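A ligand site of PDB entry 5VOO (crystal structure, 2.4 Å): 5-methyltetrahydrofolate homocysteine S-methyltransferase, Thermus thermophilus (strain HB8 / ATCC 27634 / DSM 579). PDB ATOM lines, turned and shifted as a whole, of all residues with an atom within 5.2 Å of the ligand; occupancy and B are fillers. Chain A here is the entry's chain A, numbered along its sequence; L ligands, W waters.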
ATOM      1  N   GLU A  21     -11.346 -22.224   2.821  1.00  0.00           N
ATOM      2  CA  GLU A  21     -11.636 -22.704   1.461  1.00  0.00           C
ATOM      3  C   GLU A  21     -13.124 -22.731   1.088  1.00  0.00           C
ATOM      4  O   GLU A  21     -13.422 -22.946  -0.073  1.00  0.00           O
ATOM      5  CB  GLU A  21     -11.101 -24.142   1.300  1.00  0.00           C
ATOM      6  CG  GLU A  21     -12.030 -25.238   1.817  1.00  0.00           C
ATOM      7  CD  GLU A  21     -11.441 -26.651   1.814  1.00  0.00           C
ATOM      8  OE1 GLU A  21     -10.258 -26.798   1.461  1.00  0.00           O
ATOM      9  OE2 GLU A  21     -12.186 -27.616   2.173  1.00  0.00           O
ATOM     10  N   ARG A  22     -14.042 -22.548   2.055  1.00  0.00           N
ATOM     11  CA  ARG A  22     -15.430 -22.949   1.820  1.00  0.00           C
ATOM     12  C   ARG A  22     -16.343 -21.938   1.119  1.00  0.00           C
ATOM     13  O   ARG A  22     -17.464 -22.298   0.776  1.00  0.00           O
ATOM     14  CB  ARG A  22     -16.051 -23.514   3.105  1.00  0.00           C
ATOM     15  CG  ARG A  22     -15.603 -24.937   3.377  1.00  0.00           C
ATOM     16  CD  ARG A  22     -15.871 -25.871   2.184  1.00  0.00           C
ATOM     17  NE  ARG A  22     -15.134 -27.139   2.284  1.00  0.00           N
ATOM     18  CZ  ARG A  22     -15.526 -28.186   3.014  1.00  0.00           C
ATOM     19  NH1 ARG A  22     -14.795 -29.297   3.036  1.00  0.00           N
ATOM     20  NH2 ARG A  22     -16.633 -28.125   3.717  1.00  0.00           N
ATOM     21  N   ASN A  24     -16.851 -21.220  -1.915  1.00  0.00           N
ATOM     22  CA  ASN A  24     -16.448 -21.812  -3.172  1.00  0.00           C
ATOM     23  C   ASN A  24     -17.653 -22.563  -3.717  1.00  0.00           C
ATOM     24  O   ASN A  24     -18.112 -23.533  -3.094  1.00  0.00           O
ATOM     25  CB  ASN A  24     -15.266 -22.757  -2.920  1.00  0.00           C
ATOM     26  CG  ASN A  24     -14.632 -23.256  -4.203  1.00  0.00           C
ATOM     27  OD1 ASN A  24     -15.337 -23.525  -5.171  1.00  0.00           O
ATOM     28  ND2 ASN A  24     -13.309 -23.384  -4.223  1.00  0.00           N
ATOM     29  N   THR A  26     -18.283 -24.483  -6.507  1.00  0.00           N
ATOM     30  CA  THR A  26     -18.000 -25.891  -6.832  1.00  0.00           C
ATOM     31  C   THR A  26     -17.581 -26.712  -5.637  1.00  0.00           C
ATOM     32  O   THR A  26     -17.901 -27.900  -5.584  1.00  0.00           O
ATOM     33  CB  THR A  26     -16.888 -26.042  -7.880  1.00  0.00           C
ATOM     34  OG1 THR A  26     -15.766 -25.230  -7.495  1.00  0.00           O
ATOM     35  CG2 THR A  26     -17.389 -25.579  -9.234  1.00  0.00           C
ATOM     36  N   GLY A  27     -16.878 -26.088  -4.673  1.00  0.00           N
ATOM     37  CA  GLY A  27     -16.324 -26.775  -3.498  1.00  0.00           C
ATOM     38  C   GLY A  27     -17.154 -26.815  -2.224  1.00  0.00           C
ATOM     39  O   GLY A  27     -16.702 -27.364  -1.211  1.00  0.00           O
ATOM     40  N   SER A  28     -18.344 -26.221  -2.235  1.00  0.00           N
ATOM     41  CA  SER A  28     -19.215 -26.175  -1.049  1.00  0.00           C
ATOM     42  C   SER A  28     -20.706 -26.065  -1.408  1.00  0.00           C
ATOM     43  O   SER A  28     -21.157 -25.005  -1.880  1.00  0.00           O
ATOM     44  CB  SER A  28     -18.846 -24.983  -0.170  1.00  0.00           C
ATOM     45  OG  SER A  28     -19.873 -24.677   0.778  1.00  0.00           O
ATOM     46  N   LYS A  29     -21.443 -27.146  -1.183  1.00  0.00           N
ATOM     47  CA  LYS A  29     -22.880 -27.182  -1.457  1.00  0.00           C
ATOM     48  C   LYS A  29     -23.611 -26.111  -0.631  1.00  0.00           C
ATOM     49  O   LYS A  29     -24.491 -25.413  -1.134  1.00  0.00           O
ATOM     50  CB  LYS A  29     -23.464 -28.564  -1.141  1.00  0.00           C
ATOM     51  CG  LYS A  29     -24.892 -28.710  -1.669  1.00  0.00           C
ATOM     52  CD  LYS A  29     -25.545 -30.015  -1.217  1.00  0.00           C
ATOM     53  CE  LYS A  29     -26.735 -30.338  -2.109  1.00  0.00           C
ATOM     54  NZ  LYS A  29     -27.657 -31.354  -1.507  1.00  0.00           N
ATOM     55  N   ARG A  30     -23.230 -25.998   0.642  1.00  0.00           N
ATOM     56  CA  ARG A  30     -23.783 -24.994   1.531  1.00  0.00           C
ATOM     57  C   ARG A  30     -23.603 -23.583   0.950  1.00  0.00           C
ATOM     58  O   ARG A  30     -24.557 -22.803   0.918  1.00  0.00           O
ATOM     59  CB  ARG A  30     -23.140 -25.111   2.905  1.00  0.00           C
ATOM     60  CG  ARG A  30     -23.801 -24.316   4.013  1.00  0.00           C
ATOM     61  CD  ARG A  30     -23.096 -24.522   5.360  1.00  0.00           C
ATOM     62  NE  ARG A  30     -23.320 -23.367   6.245  1.00  0.00           N
ATOM     63  CZ  ARG A  30     -22.645 -23.092   7.358  1.00  0.00           C
ATOM     64  NH1 ARG A  30     -21.668 -23.893   7.799  1.00  0.00           N
ATOM     65  NH2 ARG A  30     -22.946 -21.998   8.053  1.00  0.00           N
ATOM     66  N   ASP A  59     -10.720 -17.599   0.793  1.00  0.00           N
ATOM     67  CA  ASP A  59     -10.762 -17.856  -0.643  1.00  0.00           C
ATOM     68  C   ASP A  59     -12.194 -17.642  -1.135  1.00  0.00           C
ATOM     69  O   ASP A  59     -13.131 -18.116  -0.493  1.00  0.00           O
ATOM     70  CB  ASP A  59     -10.294 -19.280  -0.949  1.00  0.00           C
ATOM     71  CG  ASP A  59      -9.924 -19.472  -2.410  1.00  0.00           C
ATOM     72  OD1 ASP A  59      -9.091 -18.691  -2.899  1.00  0.00           O
ATOM     73  OD2 ASP A  59     -10.463 -20.413  -3.047  1.00  0.00           O
ATOM     74  N   ASP A  91     -10.404 -16.080  -6.117  1.00  0.00           N
ATOM     75  CA  ASP A  91     -10.104 -17.327  -6.809  1.00  0.00           C
ATOM     76  C   ASP A  91     -10.865 -17.283  -8.149  1.00  0.00           C
ATOM     77  O   ASP A  91     -12.076 -17.475  -8.213  1.00  0.00           O
ATOM     78  CB  ASP A  91     -10.541 -18.475  -5.912  1.00  0.00           C
ATOM     79  CG  ASP A  91     -10.068 -19.832  -6.393  1.00  0.00           C
ATOM     80  OD1 ASP A  91      -9.804 -20.004  -7.600  1.00  0.00           O
ATOM     81  OD2 ASP A  91      -9.986 -20.748  -5.544  1.00  0.00           O
ATOM     82  N   ASN A 112      -5.573 -15.096  -6.791  1.00  0.00           N
ATOM     83  CA  ASN A 112      -5.409 -16.537  -7.016  1.00  0.00           C
ATOM     84  C   ASN A 112      -6.065 -16.867  -8.362  1.00  0.00           C
ATOM     85  O   ASN A 112      -7.263 -17.100  -8.388  1.00  0.00           O
ATOM     86  CB  ASN A 112      -6.064 -17.276  -5.845  1.00  0.00           C
ATOM     87  CG  ASN A 112      -6.030 -18.784  -5.966  1.00  0.00           C
ATOM     88  OD1 ASN A 112      -5.171 -19.370  -6.619  1.00  0.00           O
ATOM     89  ND2 ASN A 112      -6.976 -19.432  -5.281  1.00  0.00           N
ATOM     90  N   VAL A 138      -0.732 -15.291  -6.053  1.00  0.00           N
ATOM     91  CA  VAL A 138      -0.516 -16.741  -6.161  1.00  0.00           C
ATOM     92  C   VAL A 138      -0.101 -17.066  -7.589  1.00  0.00           C
ATOM     93  O   VAL A 138      -0.705 -16.563  -8.531  1.00  0.00           O
ATOM     94  CB  VAL A 138      -1.778 -17.546  -5.820  1.00  0.00           C
ATOM     95  CG1 VAL A 138      -1.503 -19.058  -5.925  1.00  0.00           C
ATOM     96  CG2 VAL A 138      -2.301 -17.182  -4.438  1.00  0.00           C
ATOM     97  N   LEU A 140       0.712 -20.505 -10.083  1.00  0.00           N
ATOM     98  CA  LEU A 140       0.631 -21.964 -10.168  1.00  0.00           C
ATOM     99  C   LEU A 140       1.768 -22.470 -11.021  1.00  0.00           C
ATOM    100  O   LEU A 140       2.170 -21.803 -11.956  1.00  0.00           O
ATOM    101  CB  LEU A 140      -0.698 -22.391 -10.785  1.00  0.00           C
ATOM    102  CG  LEU A 140      -1.993 -21.831 -10.198  1.00  0.00           C
ATOM    103  CD1 LEU A 140      -3.190 -22.504 -10.883  1.00  0.00           C
ATOM    104  CD2 LEU A 140      -2.058 -22.012  -8.687  1.00  0.00           C
ATOM    105  N   ASP A 179       2.443 -21.930  -5.795  1.00  0.00           N
ATOM    106  CA  ASP A 179       1.591 -23.087  -5.610  1.00  0.00           C
ATOM    107  C   ASP A 179       2.124 -24.134  -6.553  1.00  0.00           C
ATOM    108  O   ASP A 179       1.962 -24.041  -7.765  1.00  0.00           O
ATOM    109  CB  ASP A 179       0.142 -22.747  -5.968  1.00  0.00           C
ATOM    110  CG  ASP A 179      -0.838 -23.853  -5.609  1.00  0.00           C
ATOM    111  OD1 ASP A 179      -0.447 -25.035  -5.457  1.00  0.00           O
ATOM    112  OD2 ASP A 179      -2.023 -23.527  -5.489  1.00  0.00           O
ATOM    113  N   THR A 182      -1.414 -29.411  -5.758  1.00  0.00           N
ATOM    114  CA  THR A 182      -1.817 -30.527  -4.916  1.00  0.00           C
ATOM    115  C   THR A 182      -2.782 -31.361  -5.728  1.00  0.00           C
ATOM    116  O   THR A 182      -3.835 -30.863  -6.164  1.00  0.00           O
ATOM    117  CB  THR A 182      -2.527 -30.020  -3.646  1.00  0.00           C
ATOM    118  OG1 THR A 182      -1.710 -29.039  -3.014  1.00  0.00           O
ATOM    119  CG2 THR A 182      -2.798 -31.162  -2.682  1.00  0.00           C
ATOM    120  N   VAL A 216       2.115 -21.626  -1.221  1.00  0.00           N
ATOM    121  CA  VAL A 216       0.718 -21.951  -0.851  1.00  0.00           C
ATOM    122  C   VAL A 216       0.293 -23.270  -1.454  1.00  0.00           C
ATOM    123  O   VAL A 216       0.773 -23.651  -2.507  1.00  0.00           O
ATOM    124  CB  VAL A 216      -0.269 -20.820  -1.223  1.00  0.00           C
ATOM    125  CG1 VAL A 216      -0.459 -20.684  -2.728  1.00  0.00           C
ATOM    126  CG2 VAL A 216      -1.612 -21.009  -0.520  1.00  0.00           C
ATOM    127  N   LEU A 217      -0.584 -23.989  -0.766  1.00  0.00           N
ATOM    128  CA  LEU A 217      -1.174 -25.208  -1.286  1.00  0.00           C
ATOM    129  C   LEU A 217      -2.652 -25.312  -0.974  1.00  0.00           C
ATOM    130  O   LEU A 217      -3.082 -24.906   0.105  1.00  0.00           O
ATOM    131  CB  LEU A 217      -0.474 -26.438  -0.710  1.00  0.00           C
ATOM    132  CG  LEU A 217       0.892 -26.810  -1.280  1.00  0.00           C
ATOM    133  CD1 LEU A 217       1.506 -27.922  -0.445  1.00  0.00           C
ATOM    134  CD2 LEU A 217       0.810 -27.230  -2.750  1.00  0.00           C
ATOM    135  N   GLY A 218      -3.401 -25.869  -1.924  1.00  0.00           N
ATOM    136  CA  GLY A 218      -4.787 -26.274  -1.713  1.00  0.00           C
ATOM    137  C   GLY A 218      -4.778 -27.652  -1.104  1.00  0.00           C
ATOM    138  O   GLY A 218      -4.971 -28.658  -1.803  1.00  0.00           O
ATOM    139  N   SER A 220      -6.629 -29.597   0.775  1.00  0.00           N
ATOM    140  CA  SER A 220      -7.757 -30.558   0.729  1.00  0.00           C
ATOM    141  C   SER A 220      -7.816 -31.443  -0.511  1.00  0.00           C
ATOM    142  O   SER A 220      -8.379 -32.534  -0.456  1.00  0.00           O
ATOM    143  CB  SER A 220      -9.086 -29.818   0.920  1.00  0.00           C
ATOM    144  OG  SER A 220      -9.115 -29.162   2.186  1.00  0.00           O
ATOM    145  N   ASN A 221      -7.203 -31.003  -1.616  1.00  0.00           N
ATOM    146  CA  ASN A 221      -7.189 -31.772  -2.866  1.00  0.00           C
ATOM    147  C   ASN A 221      -6.452 -33.106  -2.752  1.00  0.00           C
ATOM    148  O   ASN A 221      -6.707 -34.006  -3.555  1.00  0.00           O
ATOM    149  CB  ASN A 221      -6.534 -30.970  -3.998  1.00  0.00           C
ATOM    150  CG  ASN A 221      -7.313 -29.708  -4.354  1.00  0.00           C
ATOM    151  OD1 ASN A 221      -6.808 -28.573  -4.227  1.00  0.00           O
ATOM    152  ND2 ASN A 221      -8.523 -29.887  -4.793  1.00  0.00           N
ATOM    153  N   PHE A 224      -9.279 -36.176  -1.972  1.00  0.00           N
ATOM    154  CA  PHE A 224     -10.538 -36.444  -2.718  1.00  0.00           C
ATOM    155  C   PHE A 224     -10.850 -37.916  -2.905  1.00  0.00           C
ATOM    156  O   PHE A 224      -9.989 -38.669  -3.290  1.00  0.00           O
ATOM    157  CB  PHE A 224     -10.487 -35.819  -4.117  1.00  0.00           C
ATOM    158  CG  PHE A 224     -11.211 -34.525  -4.210  1.00  0.00           C
ATOM    159  CD1 PHE A 224     -12.598 -34.488  -4.028  1.00  0.00           C
ATOM    160  CD2 PHE A 224     -10.510 -33.335  -4.454  1.00  0.00           C
ATOM    161  CE1 PHE A 224     -13.277 -33.283  -4.091  1.00  0.00           C
ATOM    162  CE2 PHE A 224     -11.192 -32.122  -4.527  1.00  0.00           C
ATOM    163  CZ  PHE A 224     -12.582 -32.099  -4.346  1.00  0.00           C
ATOM    164  N   ARG A 231     -10.211 -37.991   5.150  1.00  0.00           N
ATOM    165  CA  ARG A 231      -9.700 -36.777   4.500  1.00  0.00           C
ATOM    166  C   ARG A 231      -9.077 -35.860   5.531  1.00  0.00           C
ATOM    167  O   ARG A 231      -7.994 -35.330   5.310  1.00  0.00           O
ATOM    168  CB  ARG A 231     -10.807 -36.061   3.711  1.00  0.00           C
ATOM    169  CG  ARG A 231     -11.315 -36.884   2.537  1.00  0.00           C
ATOM    170  CD  ARG A 231     -12.199 -36.068   1.613  1.00  0.00           C
ATOM    171  NE  ARG A 231     -11.417 -35.048   0.911  1.00  0.00           N
ATOM    172  CZ  ARG A 231     -11.919 -34.018   0.258  1.00  0.00           C
ATOM    173  NH1 ARG A 231     -13.237 -33.828   0.171  1.00  0.00           N
ATOM    174  NH2 ARG A 231     -11.091 -33.143  -0.347  1.00  0.00           N
ATOM    175  N   ILE A 251      -4.622 -23.245   1.845  1.00  0.00           N
ATOM    176  CA  ILE A 251      -6.060 -23.200   1.668  1.00  0.00           C
ATOM    177  C   ILE A 251      -6.606 -24.484   2.274  1.00  0.00           C
ATOM    178  O   ILE A 251      -6.234 -25.571   1.846  1.00  0.00           O
ATOM    179  CB  ILE A 251      -6.447 -23.076   0.189  1.00  0.00           C
ATOM    180  CG1 ILE A 251      -5.806 -21.813  -0.381  1.00  0.00           C
ATOM    181  CG2 ILE A 251      -7.952 -22.968   0.020  1.00  0.00           C
ATOM    182  CD1 ILE A 251      -5.686 -21.817  -1.889  1.00  0.00           C
HETATM  183  N1  LIG L   1      -6.435 -22.493  -5.337  1.00  0.00           N
HETATM  184  C1  LIG L   1      -5.106 -22.777  -5.296  1.00  0.00           C
HETATM  185  N2  LIG L   1      -4.216 -21.764  -5.355  1.00  0.00           N
HETATM  186  N3  LIG L   1      -4.636 -24.050  -5.212  1.00  0.00           N
HETATM  187  C2  LIG L   1      -5.447 -25.113  -5.172  1.00  0.00           C
HETATM  188  O1  LIG L   1      -4.942 -26.247  -5.108  1.00  0.00           O
HETATM  189  C3  LIG L   1      -6.914 -24.869  -5.177  1.00  0.00           C
HETATM  190  N4  LIG L   1      -7.966 -25.785  -5.242  1.00  0.00           N
HETATM  191  C4  LIG L   1      -9.259 -25.570  -4.581  1.00  0.00           C
HETATM  192  C5  LIG L   1      -9.728 -24.244  -5.217  1.00  0.00           C
HETATM  193  N5  LIG L   1      -8.689 -23.208  -5.319  1.00  0.00           N
HETATM  194  C6  LIG L   1      -7.353 -23.463  -5.294  1.00  0.00           C
HETATM  195  C7  LIG L   1      -9.077 -25.467  -3.075  1.00  0.00           C
HETATM  196  N6  LIG L   1     -10.386 -25.376  -2.449  1.00  0.00           N
HETATM  197  C8  LIG L   1      -7.927 -26.825  -6.268  1.00  0.00           C
HETATM  198  C9  LIG L   1     -12.716 -28.646  -1.516  1.00  0.00           C
HETATM  199  C10 LIG L   1     -13.207 -27.364  -1.311  1.00  0.00           C
HETATM  200  C11 LIG L   1     -12.409 -26.275  -1.633  1.00  0.00           C
HETATM  201  C12 LIG L   1     -11.143 -26.472  -2.150  1.00  0.00           C
HETATM  202  C13 LIG L   1     -10.647 -27.770  -2.350  1.00  0.00           C
HETATM  203  C14 LIG L   1     -11.436 -28.859  -2.039  1.00  0.00           C
HETATM  204  C15 LIG L   1     -13.549 -29.830  -1.176  1.00  0.00           C
HETATM  205  O2  LIG L   1     -12.962 -30.885  -1.009  1.00  0.00           O
HETATM  206  N7  LIG L   1     -14.855 -29.741  -1.036  1.00  0.00           N
HETATM  207  C16 LIG L   1     -15.639 -30.882  -0.612  1.00  0.00           C
HETATM  208  C17 LIG L   1     -16.859 -30.339   0.126  1.00  0.00           C
HETATM  209  C18 LIG L   1     -18.197 -30.979  -0.254  1.00  0.00           C
HETATM  210  C19 LIG L   1     -19.325 -30.094   0.244  1.00  0.00           C
HETATM  211  O3  LIG L   1     -19.416 -29.886   1.468  1.00  0.00           O
HETATM  212  O4  LIG L   1     -20.119 -29.610  -0.599  1.00  0.00           O
HETATM  213  C20 LIG L   1     -15.875 -31.824  -1.765  1.00  0.00           C
HETATM  214  O5  LIG L   1     -16.030 -33.055  -1.538  1.00  0.00           O
HETATM  215  O6  LIG L   1     -15.860 -31.357  -2.942  1.00  0.00           O
HETATM  216  O   HOH W   1      -2.294 -26.642  -4.474  1.00  0.00           O
HETATM  217  O   HOH W   2     -11.562 -22.559  -2.139  1.00  0.00           O
HETATM  218  O   HOH W   3     -12.519 -30.239   1.866  1.00  0.00           O
HETATM  219  O   HOH W   4     -10.523 -22.823  -8.219  1.00  0.00           O
HETATM  220  O   HOH W   5     -12.571 -23.986  -7.111  1.00  0.00           O
HETATM  221  O   HOH W   6      -3.687 -27.949  -7.041  1.00  0.00           O
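A nitrogen (N5) of the ligand lies within hydrogen-bond range of the side-chain carboxylate (OD2) of Asp 91, at 2.8 Å.
The guanidinium group (NH1) of Arg 231 lies within salt-bridge range of an oxygen (O5) of the ligand, at 3.4 Å.
OD1 of Asn 112 lies within hydrogen-bond range of N2 of the ligand, at 2.9 Å.
An oxygen (O3) of the ligand is in salt-bridge range of the guanidinium group (NH2) of Arg 22 (3.99 Å).
The side-chain amide oxygen (OD1) of Asn 221 lies close to an oxygen (O1) of the ligand, 3.1 Å away.
N of Lys 29 sits at hydrogen-bond distance from O4 of the ligand (2.9 Å).
The side-chain carboxylate (OD2) of Asp 179 lies within hydrogen-bond range of a nitrogen (N3) of the ligand (2.7 Å).
A nitrogen (N7) of the ligand lies within hydrogen-bond range of the backbone carbonyl oxygen (O) of Gly 27, at 3.0 Å.
The side-chain hydroxyl (OG) of Ser 28 lies close to the backbone carbonyl oxygen (O) of Arg 22 (3.4 Å).
The side-chain carboxylate of Asp 91 lies close to the side-chain carboxylate of Asp 59 (2.6 Å).
OG of Ser 220 is in hydrogen-bond range of OE1 of Glu 21.
O of Gly 218 sits close to OD1 of Asn 221 (3.0 Å).
NH2 of Arg 231 is in hydrogen-bond range of O of Ser 220, 2.8 Å away.
OD2 of Asp 91 sits at hydrogen-bond distance from ND2 of Asn 112, at 3.3 Å.
O of Gly 218 lies close to OG1 of Thr 182 (3.5 Å).
N of Gly 27 sits at hydrogen-bond distance from OD1 of Asn 24, at 3.0 Å.
Merely in contact with the ligand: Glu 21 (3.6 Å), Asn 24 (3.8 Å), Ser 28 (3.6 Å), Val 138 (3.9 Å), Leu 140 (3.98 Å), Gly 218 (3.4 Å), Ser 220 (3.9 Å), Phe 224 (3.4 Å) and Ile 251 (3.6 Å).
The nearest printed residue that does not touch the ligand is Asp 59 (4.02 Å).
Water W1 lies within hydrogen-bond range of OD1 of Asp 179 (2.6 Å), O1 of the ligand (2.8 Å), OG1 of Thr 182 (2.9 Å) and N of Gly 218 (2.9 Å).
Water W6 lies within hydrogen-bond range of O1 of the ligand (2.9 Å) and N of Thr 182 (3.0 Å).
Water W3 lies within hydrogen-bond range of OE2 of Glu 21 (2.7 Å), NH1 of Arg 22 (2.7 Å) and O2 of the ligand (3.0 Å).
Water W2 lies within hydrogen-bond range of the side-chain carboxylate (OD2) of Asp 59 (2.6 Å), the backbone carbonyl oxygen (O) of Glu 21 (2.8 Å), the side-chain amide nitrogen (ND2) of Asn 24 (2.8 Å) and a nitrogen (N6) of the ligand (3.1 Å).
Water W4 bridges OD1 of Asp 91 (3.0 Å) and N5 of the ligand (3.5 Å).
Water W5 bridges the side-chain amide nitrogen of Asn 24 (3.0 Å) and the side-chain hydroxyl of Thr 26 (3.5 Å).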
